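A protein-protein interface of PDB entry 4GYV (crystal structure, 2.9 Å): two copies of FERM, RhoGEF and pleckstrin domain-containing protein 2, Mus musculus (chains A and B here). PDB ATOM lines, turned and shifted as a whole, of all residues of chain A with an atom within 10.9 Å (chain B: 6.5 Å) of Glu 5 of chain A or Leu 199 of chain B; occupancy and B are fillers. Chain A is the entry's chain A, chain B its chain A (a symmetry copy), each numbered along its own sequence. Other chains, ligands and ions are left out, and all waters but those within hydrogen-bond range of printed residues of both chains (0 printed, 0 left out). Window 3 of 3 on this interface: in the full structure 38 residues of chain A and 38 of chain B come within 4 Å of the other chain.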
ATOM      1  N   GLY A   1     -17.476  34.498 -16.250  1.00  0.00           N
ATOM      2  CA  GLY A   1     -16.057  34.184 -16.262  1.00  0.00           C
ATOM      3  C   GLY A   1     -15.770  32.700 -16.422  1.00  0.00           C
ATOM      4  O   GLY A   1     -16.664  31.935 -16.776  1.00  0.00           O
ATOM      5  N   PRO A   2     -14.508  32.288 -16.176  1.00  0.00           N
ATOM      6  CA  PRO A   2     -14.122  30.872 -16.169  1.00  0.00           C
ATOM      7  C   PRO A   2     -14.444  30.274 -14.819  1.00  0.00           C
ATOM      8  O   PRO A   2     -14.507  31.016 -13.829  1.00  0.00           O
ATOM      9  CB  PRO A   2     -12.608  30.928 -16.330  1.00  0.00           C
ATOM     10  CG  PRO A   2     -12.210  32.219 -15.697  1.00  0.00           C
ATOM     11  CD  PRO A   2     -13.349  33.176 -15.941  1.00  0.00           C
ATOM     12  N   HIS A   3     -14.665  28.965 -14.764  1.00  0.00           N
ATOM     13  CA  HIS A   3     -14.867  28.317 -13.472  1.00  0.00           C
ATOM     14  C   HIS A   3     -13.496  28.183 -12.835  1.00  0.00           C
ATOM     15  O   HIS A   3     -12.513  27.882 -13.515  1.00  0.00           O
ATOM     16  CB  HIS A   3     -15.553  26.956 -13.598  1.00  0.00           C
ATOM     17  CG  HIS A   3     -15.777  26.284 -12.282  1.00  0.00           C
ATOM     18  ND1 HIS A   3     -14.901  25.354 -11.763  1.00  0.00           N
ATOM     19  CD2 HIS A   3     -16.761  26.430 -11.362  1.00  0.00           C
ATOM     20  CE1 HIS A   3     -15.341  24.949 -10.585  1.00  0.00           C
ATOM     21  NE2 HIS A   3     -16.471  25.582 -10.320  1.00  0.00           N
ATOM     22  N   MET A   4     -13.420  28.422 -11.536  1.00  0.00           N
ATOM     23  CA  MET A   4     -12.119  28.631 -10.926  1.00  0.00           C
ATOM     24  C   MET A   4     -11.181  27.435 -10.895  1.00  0.00           C
ATOM     25  O   MET A   4      -9.973  27.621 -10.729  1.00  0.00           O
ATOM     26  CB  MET A   4     -12.279  29.238  -9.551  1.00  0.00           C
ATOM     27  CG  MET A   4     -12.842  30.631  -9.647  1.00  0.00           C
ATOM     28  SD  MET A   4     -13.224  31.389  -7.904  1.00  0.00           S
ATOM     29  CE  MET A   4     -11.393  31.455  -7.210  1.00  0.00           C
ATOM     30  N   GLU A   5     -11.714  26.223 -11.076  1.00  0.00           N
ATOM     31  CA  GLU A   5     -10.871  25.025 -11.079  1.00  0.00           C
ATOM     32  C   GLU A   5     -10.789  24.350 -12.456  1.00  0.00           C
ATOM     33  O   GLU A   5     -10.325  23.214 -12.575  1.00  0.00           O
ATOM     34  CB  GLU A   5     -11.323  24.045  -9.996  1.00  0.00           C
ATOM     35  CG  GLU A   5     -11.492  24.689  -8.629  1.00  0.00           C
ATOM     36  CD  GLU A   5     -11.691  23.677  -7.514  1.00  0.00           C
ATOM     37  OE1 GLU A   5     -12.865  23.427  -7.132  1.00  0.00           O
ATOM     38  OE2 GLU A   5     -10.663  23.147  -7.018  1.00  0.00           O
ATOM     39  N   ASP A   6     -11.229  25.076 -13.486  1.00  0.00           N
ATOM     40  CA  ASP A   6     -11.225  24.625 -14.885  1.00  0.00           C
ATOM     41  C   ASP A   6      -9.812  24.486 -15.467  1.00  0.00           C
ATOM     42  O   ASP A   6      -9.155  25.493 -15.761  1.00  0.00           O
ATOM     43  CB  ASP A   6     -12.006  25.645 -15.722  1.00  0.00           C
ATOM     44  CG  ASP A   6     -12.258  25.189 -17.160  1.00  0.00           C
ATOM     45  OD1 ASP A   6     -11.822  24.084 -17.561  1.00  0.00           O
ATOM     46  OD2 ASP A   6     -12.917  25.965 -17.893  1.00  0.00           O
ATOM     47  N   GLU A   7      -9.357  23.252 -15.664  1.00  0.00           N
ATOM     48  CA  GLU A   7      -8.022  23.051 -16.202  1.00  0.00           C
ATOM     49  C   GLU A   7      -7.894  23.535 -17.654  1.00  0.00           C
ATOM     50  O   GLU A   7      -6.828  24.003 -18.079  1.00  0.00           O
ATOM     51  CB  GLU A   7      -7.561  21.601 -16.052  1.00  0.00           C
ATOM     52  CG  GLU A   7      -6.125  21.401 -16.516  1.00  0.00           C
ATOM     53  CD  GLU A   7      -5.536  20.061 -16.112  1.00  0.00           C
ATOM     54  OE1 GLU A   7      -4.432  19.739 -16.640  1.00  0.00           O
ATOM     55  OE2 GLU A   7      -6.168  19.354 -15.272  1.00  0.00           O
ATOM     56  N   ALA A   8      -8.978  23.448 -18.412  1.00  0.00           N
ATOM     57  CA  ALA A   8      -8.922  23.938 -19.778  1.00  0.00           C
ATOM     58  C   ALA A   8      -8.664  25.436 -19.768  1.00  0.00           C
ATOM     59  O   ALA A   8      -7.849  25.919 -20.548  1.00  0.00           O
ATOM     60  CB  ALA A   8     -10.178  23.595 -20.548  1.00  0.00           C
ATOM     61  N   TYR A   9      -9.323  26.173 -18.869  1.00  0.00           N
ATOM     62  CA  TYR A   9      -9.075  27.613 -18.789  1.00  0.00           C
ATOM     63  C   TYR A   9      -7.596  27.893 -18.489  1.00  0.00           C
ATOM     64  O   TYR A   9      -6.975  28.712 -19.160  1.00  0.00           O
ATOM     65  CB  TYR A   9     -10.007  28.349 -17.806  1.00  0.00           C
ATOM     66  CG  TYR A   9      -9.547  29.773 -17.573  1.00  0.00           C
ATOM     67  CD1 TYR A   9      -9.719  30.739 -18.540  1.00  0.00           C
ATOM     68  CD2 TYR A   9      -8.872  30.131 -16.414  1.00  0.00           C
ATOM     69  CE1 TYR A   9      -9.248  32.032 -18.353  1.00  0.00           C
ATOM     70  CE2 TYR A   9      -8.408  31.415 -16.222  1.00  0.00           C
ATOM     71  CZ  TYR A   9      -8.593  32.367 -17.190  1.00  0.00           C
ATOM     72  OH  TYR A   9      -8.116  33.657 -17.001  1.00  0.00           O
ATOM     73  N   PHE A  10      -7.024  27.195 -17.509  1.00  0.00           N
ATOM     74  CA  PHE A  10      -5.611  27.393 -17.178  1.00  0.00           C
ATOM     75  C   PHE A  10      -4.662  27.129 -18.345  1.00  0.00           C
ATOM     76  O   PHE A  10      -3.752  27.898 -18.584  1.00  0.00           O
ATOM     77  CB  PHE A  10      -5.199  26.584 -15.964  1.00  0.00           C
ATOM     78  CG  PHE A  10      -5.866  27.022 -14.686  1.00  0.00           C
ATOM     79  CD1 PHE A  10      -5.738  28.322 -14.230  1.00  0.00           C
ATOM     80  CD2 PHE A  10      -6.601  26.123 -13.917  1.00  0.00           C
ATOM     81  CE1 PHE A  10      -6.348  28.729 -13.044  1.00  0.00           C
ATOM     82  CE2 PHE A  10      -7.205  26.522 -12.729  1.00  0.00           C
ATOM     83  CZ  PHE A  10      -7.089  27.828 -12.298  1.00  0.00           C
ATOM     84  N   ILE A  11      -4.879  26.060 -19.093  1.00  0.00           N
ATOM     85  CA  ILE A  11      -4.012  25.790 -20.233  1.00  0.00           C
ATOM     86  C   ILE A  11      -4.129  26.913 -21.245  1.00  0.00           C
ATOM     87  O   ILE A  11      -3.125  27.413 -21.737  1.00  0.00           O
ATOM     88  CB  ILE A  11      -4.336  24.451 -20.893  1.00  0.00           C
ATOM     89  CG1 ILE A  11      -4.073  23.320 -19.927  1.00  0.00           C
ATOM     90  CG2 ILE A  11      -3.508  24.246 -22.147  1.00  0.00           C
ATOM     91  CD1 ILE A  11      -4.764  22.053 -20.350  1.00  0.00           C
ATOM     92  N   GLU A  14      -2.214  29.743 -19.982  1.00  0.00           N
ATOM     93  CA  GLU A  14      -0.796  29.420 -20.100  1.00  0.00           C
ATOM     94  C   GLU A  14      -0.318  29.607 -21.553  1.00  0.00           C
ATOM     95  O   GLU A  14       0.772  30.122 -21.796  1.00  0.00           O
ATOM     96  CB  GLU A  14      -0.502  27.990 -19.591  1.00  0.00           C
ATOM     97  CG  GLU A  14      -0.544  27.803 -18.048  1.00  0.00           C
ATOM     98  CD  GLU A  14      -0.663  26.321 -17.589  1.00  0.00           C
ATOM     99  OE1 GLU A  14      -0.593  25.414 -18.454  1.00  0.00           O
ATOM    100  OE2 GLU A  14      -0.810  26.054 -16.361  1.00  0.00           O
ATOM    101  N   TRP A  76     -13.722  34.616 -22.782  1.00  0.00           N
ATOM    102  CA  TRP A  76     -13.804  33.513 -21.841  1.00  0.00           C
ATOM    103  C   TRP A  76     -13.840  34.068 -20.417  1.00  0.00           C
ATOM    104  O   TRP A  76     -14.697  33.686 -19.621  1.00  0.00           O
ATOM    105  CB  TRP A  76     -12.599  32.597 -22.058  1.00  0.00           C
ATOM    106  CG  TRP A  76     -12.675  31.271 -21.396  1.00  0.00           C
ATOM    107  CD1 TRP A  76     -13.337  30.959 -20.251  1.00  0.00           C
ATOM    108  CD2 TRP A  76     -12.039  30.065 -21.835  1.00  0.00           C
ATOM    109  NE1 TRP A  76     -13.158  29.630 -19.946  1.00  0.00           N
ATOM    110  CE2 TRP A  76     -12.368  29.056 -20.902  1.00  0.00           C
ATOM    111  CE3 TRP A  76     -11.230  29.738 -22.928  1.00  0.00           C
ATOM    112  CZ2 TRP A  76     -11.921  27.742 -21.029  1.00  0.00           C
ATOM    113  CZ3 TRP A  76     -10.787  28.430 -23.061  1.00  0.00           C
ATOM    114  CH2 TRP A  76     -11.130  27.448 -22.108  1.00  0.00           C
ATOM    115  N   HIS A 170      -7.248  16.245 -21.110  1.00  0.00           N
ATOM    116  CA  HIS A 170      -8.185  16.766 -20.131  1.00  0.00           C
ATOM    117  C   HIS A 170      -9.641  16.560 -20.541  1.00  0.00           C
ATOM    118  O   HIS A 170     -10.476  16.140 -19.740  1.00  0.00           O
ATOM    119  CB  HIS A 170      -7.923  18.249 -19.895  1.00  0.00           C
ATOM    120  CG  HIS A 170      -9.068  18.956 -19.246  1.00  0.00           C
ATOM    121  ND1 HIS A 170      -9.369  18.806 -17.910  1.00  0.00           N
ATOM    122  CD2 HIS A 170     -10.007  19.789 -19.755  1.00  0.00           C
ATOM    123  CE1 HIS A 170     -10.434  19.535 -17.620  1.00  0.00           C
ATOM    124  NE2 HIS A 170     -10.842  20.140 -18.723  1.00  0.00           N
ATOM    125  N   TYR A 171      -9.933  16.868 -21.796  1.00  0.00           N
ATOM    126  CA  TYR A 171     -11.288  16.800 -22.326  1.00  0.00           C
ATOM    127  C   TYR A 171     -11.749  15.354 -22.461  1.00  0.00           C
ATOM    128  O   TYR A 171     -10.960  14.456 -22.799  1.00  0.00           O
ATOM    129  CB  TYR A 171     -11.346  17.496 -23.688  1.00  0.00           C
ATOM    130  CG  TYR A 171     -11.357  19.017 -23.635  1.00  0.00           C
ATOM    131  CD1 TYR A 171     -12.252  19.692 -22.818  1.00  0.00           C
ATOM    132  CD2 TYR A 171     -10.499  19.778 -24.422  1.00  0.00           C
ATOM    133  CE1 TYR A 171     -12.291  21.072 -22.771  1.00  0.00           C
ATOM    134  CE2 TYR A 171     -10.532  21.174 -24.377  1.00  0.00           C
ATOM    135  CZ  TYR A 171     -11.439  21.807 -23.541  1.00  0.00           C
ATOM    136  OH  TYR A 171     -11.520  23.176 -23.460  1.00  0.00           O
ATOM    137  N   GLN B 110      -8.780  34.688   2.686  1.00  0.00           N
ATOM    138  CA  GLN B 110      -9.981  34.269   3.381  1.00  0.00           C
ATOM    139  C   GLN B 110     -11.045  35.366   3.460  1.00  0.00           C
ATOM    140  O   GLN B 110     -12.216  35.069   3.620  1.00  0.00           O
ATOM    141  CB  GLN B 110      -9.616  33.813   4.788  1.00  0.00           C
ATOM    142  CG  GLN B 110     -10.584  32.869   5.379  1.00  0.00           C
ATOM    143  CD  GLN B 110     -10.134  31.455   5.204  1.00  0.00           C
ATOM    144  OE1 GLN B 110      -9.176  31.028   5.852  1.00  0.00           O
ATOM    145  NE2 GLN B 110     -10.814  30.703   4.325  1.00  0.00           N
ATOM    146  N   ASP B 113     -14.162  36.803  -0.250  1.00  0.00           N
ATOM    147  CA  ASP B 113     -15.584  36.634  -0.530  1.00  0.00           C
ATOM    148  C   ASP B 113     -16.399  37.655   0.256  1.00  0.00           C
ATOM    149  O   ASP B 113     -17.469  38.106  -0.177  1.00  0.00           O
ATOM    150  CB  ASP B 113     -16.025  35.219  -0.183  1.00  0.00           C
ATOM    151  CG  ASP B 113     -15.774  34.880   1.268  1.00  0.00           C
ATOM    152  OD1 ASP B 113     -14.592  34.684   1.635  1.00  0.00           O
ATOM    153  OD2 ASP B 113     -16.757  34.811   2.040  1.00  0.00           O
ATOM    154  N   VAL B 154      -7.481  33.986  -5.340  1.00  0.00           N
ATOM    155  CA  VAL B 154      -7.699  32.607  -4.914  1.00  0.00           C
ATOM    156  C   VAL B 154      -7.583  31.630  -6.092  1.00  0.00           C
ATOM    157  O   VAL B 154      -7.013  30.553  -5.977  1.00  0.00           O
ATOM    158  CB  VAL B 154      -9.020  32.438  -4.143  1.00  0.00           C
ATOM    159  CG1 VAL B 154      -9.256  30.988  -3.810  1.00  0.00           C
ATOM    160  CG2 VAL B 154      -8.965  33.231  -2.863  1.00  0.00           C
ATOM    161  N   GLN B 155      -8.093  32.023  -7.243  1.00  0.00           N
ATOM    162  CA  GLN B 155      -7.869  31.243  -8.445  1.00  0.00           C
ATOM    163  C   GLN B 155      -6.377  31.014  -8.738  1.00  0.00           C
ATOM    164  O   GLN B 155      -6.005  29.955  -9.221  1.00  0.00           O
ATOM    165  CB  GLN B 155      -8.566  31.902  -9.622  1.00  0.00           C
ATOM    166  CG  GLN B 155      -8.360  31.194 -10.936  1.00  0.00           C
ATOM    167  CD  GLN B 155      -9.070  31.888 -12.087  1.00  0.00           C
ATOM    168  OE1 GLN B 155      -9.354  33.091 -12.035  1.00  0.00           O
ATOM    169  NE2 GLN B 155      -9.362  31.129 -13.133  1.00  0.00           N
ATOM    170  N   VAL B 158      -5.026  28.083  -6.773  1.00  0.00           N
ATOM    171  CA  VAL B 158      -5.437  26.815  -7.343  1.00  0.00           C
ATOM    172  C   VAL B 158      -4.518  26.458  -8.493  1.00  0.00           C
ATOM    173  O   VAL B 158      -4.060  25.326  -8.611  1.00  0.00           O
ATOM    174  CB  VAL B 158      -6.865  26.913  -7.866  1.00  0.00           C
ATOM    175  CG1 VAL B 158      -7.187  25.736  -8.765  1.00  0.00           C
ATOM    176  CG2 VAL B 158      -7.819  26.991  -6.710  1.00  0.00           C
ATOM    177  N   ARG B 161      -1.359  24.953  -7.283  1.00  0.00           N
ATOM    178  CA  ARG B 161      -1.490  23.549  -6.900  1.00  0.00           C
ATOM    179  C   ARG B 161      -1.403  22.697  -8.157  1.00  0.00           C
ATOM    180  O   ARG B 161      -0.853  21.603  -8.142  1.00  0.00           O
ATOM    181  CB  ARG B 161      -2.811  23.284  -6.164  1.00  0.00           C
ATOM    182  CG  ARG B 161      -2.908  21.910  -5.461  1.00  0.00           C
ATOM    183  CD  ARG B 161      -4.278  21.225  -5.634  1.00  0.00           C
ATOM    184  NE  ARG B 161      -5.412  21.990  -5.091  1.00  0.00           N
ATOM    185  CZ  ARG B 161      -6.510  22.317  -5.784  1.00  0.00           C
ATOM    186  NH1 ARG B 161      -6.629  21.954  -7.060  1.00  0.00           N
ATOM    187  NH2 ARG B 161      -7.492  23.011  -5.210  1.00  0.00           N
ATOM    188  N   LEU B 162      -1.936  23.222  -9.250  1.00  0.00           N
ATOM    189  CA  LEU B 162      -1.996  22.498 -10.504  1.00  0.00           C
ATOM    190  C   LEU B 162      -0.613  22.331 -11.074  1.00  0.00           C
ATOM    191  O   LEU B 162      -0.215  21.228 -11.454  1.00  0.00           O
ATOM    192  CB  LEU B 162      -2.822  23.297 -11.493  1.00  0.00           C
ATOM    193  CG  LEU B 162      -4.178  22.729 -11.824  1.00  0.00           C
ATOM    194  CD1 LEU B 162      -3.916  21.562 -12.765  1.00  0.00           C
ATOM    195  CD2 LEU B 162      -4.903  22.314 -10.511  1.00  0.00           C
ATOM    196  N   THR B 192      -4.689  25.704  -0.132  1.00  0.00           N
ATOM    197  CA  THR B 192      -5.941  25.569  -0.851  1.00  0.00           C
ATOM    198  C   THR B 192      -6.978  24.835   0.005  1.00  0.00           C
ATOM    199  O   THR B 192      -8.141  25.212   0.034  1.00  0.00           O
ATOM    200  CB  THR B 192      -5.751  24.867  -2.198  1.00  0.00           C
ATOM    201  OG1 THR B 192      -5.172  23.580  -1.990  1.00  0.00           O
ATOM    202  CG2 THR B 192      -4.834  25.660  -3.079  1.00  0.00           C
ATOM    203  N   LEU B 195      -8.519  27.179   2.336  1.00  0.00           N
ATOM    204  CA  LEU B 195      -9.308  28.197   1.678  1.00  0.00           C
ATOM    205  C   LEU B 195     -10.477  27.586   0.926  1.00  0.00           C
ATOM    206  O   LEU B 195     -11.199  28.295   0.242  1.00  0.00           O
ATOM    207  CB  LEU B 195      -8.442  29.003   0.710  1.00  0.00           C
ATOM    208  CG  LEU B 195      -7.388  29.946   1.289  1.00  0.00           C
ATOM    209  CD1 LEU B 195      -6.557  30.524   0.180  1.00  0.00           C
ATOM    210  CD2 LEU B 195      -8.020  31.070   2.082  1.00  0.00           C
ATOM    211  N   GLN B 196     -10.661  26.275   1.051  1.00  0.00           N
ATOM    212  CA  GLN B 196     -11.708  25.578   0.297  1.00  0.00           C
ATOM    213  C   GLN B 196     -13.064  26.250   0.460  1.00  0.00           C
ATOM    214  O   GLN B 196     -13.742  26.544  -0.531  1.00  0.00           O
ATOM    215  CB  GLN B 196     -11.785  24.090   0.683  1.00  0.00           C
ATOM    216  CG  GLN B 196     -12.651  23.228  -0.229  1.00  0.00           C
ATOM    217  CD  GLN B 196     -12.333  23.402  -1.717  1.00  0.00           C
ATOM    218  OE1 GLN B 196     -13.235  23.645  -2.532  1.00  0.00           O
ATOM    219  NE2 GLN B 196     -11.050  23.262  -2.081  1.00  0.00           N
ATOM    220  N   GLN B 197     -13.432  26.523   1.707  1.00  0.00           N
ATOM    221  CA  GLN B 197     -14.719  27.135   1.994  1.00  0.00           C
ATOM    222  C   GLN B 197     -14.839  28.447   1.240  1.00  0.00           C
ATOM    223  O   GLN B 197     -15.827  28.670   0.539  1.00  0.00           O
ATOM    224  CB  GLN B 197     -14.883  27.371   3.493  1.00  0.00           C
ATOM    225  CG  GLN B 197     -16.202  26.888   4.082  1.00  0.00           C
ATOM    226  CD  GLN B 197     -16.301  27.164   5.582  1.00  0.00           C
ATOM    227  OE1 GLN B 197     -15.708  28.123   6.095  1.00  0.00           O
ATOM    228  NE2 GLN B 197     -17.043  26.315   6.294  1.00  0.00           N
ATOM    229  N   SER B 198     -13.820  29.295   1.371  1.00  0.00           N
ATOM    230  CA  SER B 198     -13.834  30.620   0.763  1.00  0.00           C
ATOM    231  C   SER B 198     -13.821  30.516  -0.749  1.00  0.00           C
ATOM    232  O   SER B 198     -14.419  31.339  -1.453  1.00  0.00           O
ATOM    233  CB  SER B 198     -12.645  31.459   1.248  1.00  0.00           C
ATOM    234  OG  SER B 198     -12.883  31.970   2.547  1.00  0.00           O
ATOM    235  N   LEU B 199     -13.124  29.503  -1.246  1.00  0.00           N
ATOM    236  CA  LEU B 199     -13.055  29.251  -2.677  1.00  0.00           C
ATOM    237  C   LEU B 199     -14.471  29.028  -3.221  1.00  0.00           C
ATOM    238  O   LEU B 199     -14.929  29.819  -4.060  1.00  0.00           O
ATOM    239  CB  LEU B 199     -12.132  28.056  -2.976  1.00  0.00           C
ATOM    240  CG  LEU B 199     -12.126  27.418  -4.377  1.00  0.00           C
ATOM    241  CD1 LEU B 199     -11.631  28.398  -5.430  1.00  0.00           C
ATOM    242  CD2 LEU B 199     -11.315  26.103  -4.399  1.00  0.00           C
ATOM    243  N   THR B 200     -15.174  27.995  -2.723  1.00  0.00           N
ATOM    244  CA  THR B 200     -16.503  27.692  -3.257  1.00  0.00           C
ATOM    245  C   THR B 200     -17.481  28.829  -2.990  1.00  0.00           C
ATOM    246  O   THR B 200     -18.442  29.009  -3.730  1.00  0.00           O
ATOM    247  CB  THR B 200     -17.127  26.317  -2.789  1.00  0.00           C
ATOM    248  OG1 THR B 200     -17.731  26.459  -1.512  1.00  0.00           O
ATOM    249  CG2 THR B 200     -16.108  25.170  -2.750  1.00  0.00           C
ATOM    250  N   ARG B 201     -17.236  29.609  -1.947  1.00  0.00           N
ATOM    251  CA  ARG B 201     -18.089  30.753  -1.682  1.00  0.00           C
ATOM    252  C   ARG B 201     -17.924  31.750  -2.821  1.00  0.00           C
ATOM    253  O   ARG B 201     -18.896  32.356  -3.272  1.00  0.00           O
ATOM    254  CB  ARG B 201     -17.743  31.384  -0.343  1.00  0.00           C
ATOM    255  CG  ARG B 201     -18.930  31.905   0.435  1.00  0.00           C
ATOM    256  CD  ARG B 201     -19.018  31.217   1.792  1.00  0.00           C
ATOM    257  NE  ARG B 201     -17.763  31.305   2.545  1.00  0.00           N
ATOM    258  CZ  ARG B 201     -17.556  30.776   3.752  1.00  0.00           C
ATOM    259  NH1 ARG B 201     -18.529  30.113   4.371  1.00  0.00           N
ATOM    260  NH2 ARG B 201     -16.366  30.913   4.339  1.00  0.00           N
ATOM    261  N   LEU B 202     -16.688  31.886  -3.303  1.00  0.00           N
ATOM    262  CA  LEU B 202     -16.369  32.829  -4.372  1.00  0.00           C
ATOM    263  C   LEU B 202     -16.889  32.340  -5.726  1.00  0.00           C
ATOM    264  O   LEU B 202     -17.469  33.114  -6.483  1.00  0.00           O
ATOM    265  CB  LEU B 202     -14.863  33.109  -4.406  1.00  0.00           C
ATOM    266  CG  LEU B 202     -14.340  34.180  -3.427  1.00  0.00           C
ATOM    267  CD1 LEU B 202     -12.864  33.972  -3.142  1.00  0.00           C
ATOM    268  CD2 LEU B 202     -14.583  35.627  -3.896  1.00  0.00           C
ATOM    269  N   GLU B 203     -16.698  31.055  -6.018  1.00  0.00           N
ATOM    270  CA  GLU B 203     -17.379  30.413  -7.141  1.00  0.00           C
ATOM    271  C   GLU B 203     -18.887  30.759  -7.131  1.00  0.00           C
ATOM    272  O   GLU B 203     -19.378  31.408  -8.060  1.00  0.00           O
ATOM    273  CB  GLU B 203     -17.168  28.883  -7.115  1.00  0.00           C
ATOM    274  CG  GLU B 203     -15.739  28.391  -7.463  1.00  0.00           C
ATOM    275  CD  GLU B 203     -15.506  26.871  -7.232  1.00  0.00           C
ATOM    276  OE1 GLU B 203     -16.446  26.128  -6.871  1.00  0.00           O
ATOM    277  OE2 GLU B 203     -14.356  26.414  -7.413  1.00  0.00           O
ATOM    278  N   ASN B 204     -19.605  30.365  -6.072  1.00  0.00           N
ATOM    279  CA  ASN B 204     -21.044  30.647  -5.970  1.00  0.00           C
ATOM    280  C   ASN B 204     -21.408  32.113  -6.201  1.00  0.00           C
ATOM    281  O   ASN B 204     -22.360  32.423  -6.932  1.00  0.00           O
ATOM    282  CB  ASN B 204     -21.609  30.184  -4.636  1.00  0.00           C
ATOM    283  CG  ASN B 204     -21.522  28.686  -4.458  1.00  0.00           C
ATOM    284  OD1 ASN B 204     -20.984  27.985  -5.313  1.00  0.00           O
ATOM    285  ND2 ASN B 204     -22.032  28.185  -3.333  1.00  0.00           N
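The side-chain carboxylate (OE1) of Glu 5 of chain A sits close to the side-chain carboxylate (OE2) of Glu 203 of chain B, 3.4 Å away. The side-chain carboxylate (OE2) of Glu 5 of chain A lies within salt-bridge range of the guanidinium group (NH2) of Arg 161 of chain B (3.7 Å). The side-chain carboxylate (OE1) of Glu 203 of chain B sits close to a ring nitrogen (NE2) of His 3 of chain A, at 3.5 Å.
The guanidinium group (NE) of Arg 161 of chain B is in hydrogen-bond range of the side-chain hydroxyl (OG1) of Thr 192 of chain B (3.5 Å). N of Glu 5 of chain A sits close to ND1 of His 3 of chain A.
Among the printed residues, pairs that only touch across the chains: Tyr 9 of chain A with Gln 155 of chain B, Met 4 of chain A with Gln 155 of chain B, Met 4 of chain A with Leu 199 of chain B, Phe 10 of chain A with Gln 155 of chain B, Met 4 of chain A with Val 158 of chain B, Met 4 of chain A with Glu 203 of chain B, Glu 5 of chain A with Leu 199 of chain B, Met 4 of chain A with Val 154 of chain B and Pro 2 of chain A with Gln 155 of chain B.
Of chain B, only Arg 161, Leu 199 and Glu 203 come within 4 Å of Glu 5 of chain A. Of the printed residues of chain B, Phe 10 of chain A touches Gln 155 (3.8 Å). Of the printed residues of chain A, Val 158 of chain B touches Met 4. Leu 195 of chain B touches none of the printed residues of chain A. Ser 198 of chain B touches none of the printed residues of chain A. No residue of chain A comes within 4 Å of Thr 200 of chain B. No residue of chain A comes within 4 Å of Leu 202 of chain B. Of the printed residues of chain A, Glu 203 of chain B touches His 3 (3.5 Å), Met 4 (3.9 Å) and Glu 5 (3.4 Å).
Hydrophobic or aromatic side chains of chain A that line the printed part of chain B: Pro 2, His 3, Met 4, Tyr 9 and Phe 10. Of the 18 printed residues of chain B, 6 touch a printed residue of chain A. Among the printed residues, Asp or Glu carboxylates within 4 Å of a Lys or Arg side-chain nitrogen of the other chain: Glu 5 of chain A with Arg 161 of chain B.
No position is printed for both chains. Of the 12 pairs that touch across the chains among the printed residues, none has its exchanged pair printed and touching as well.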
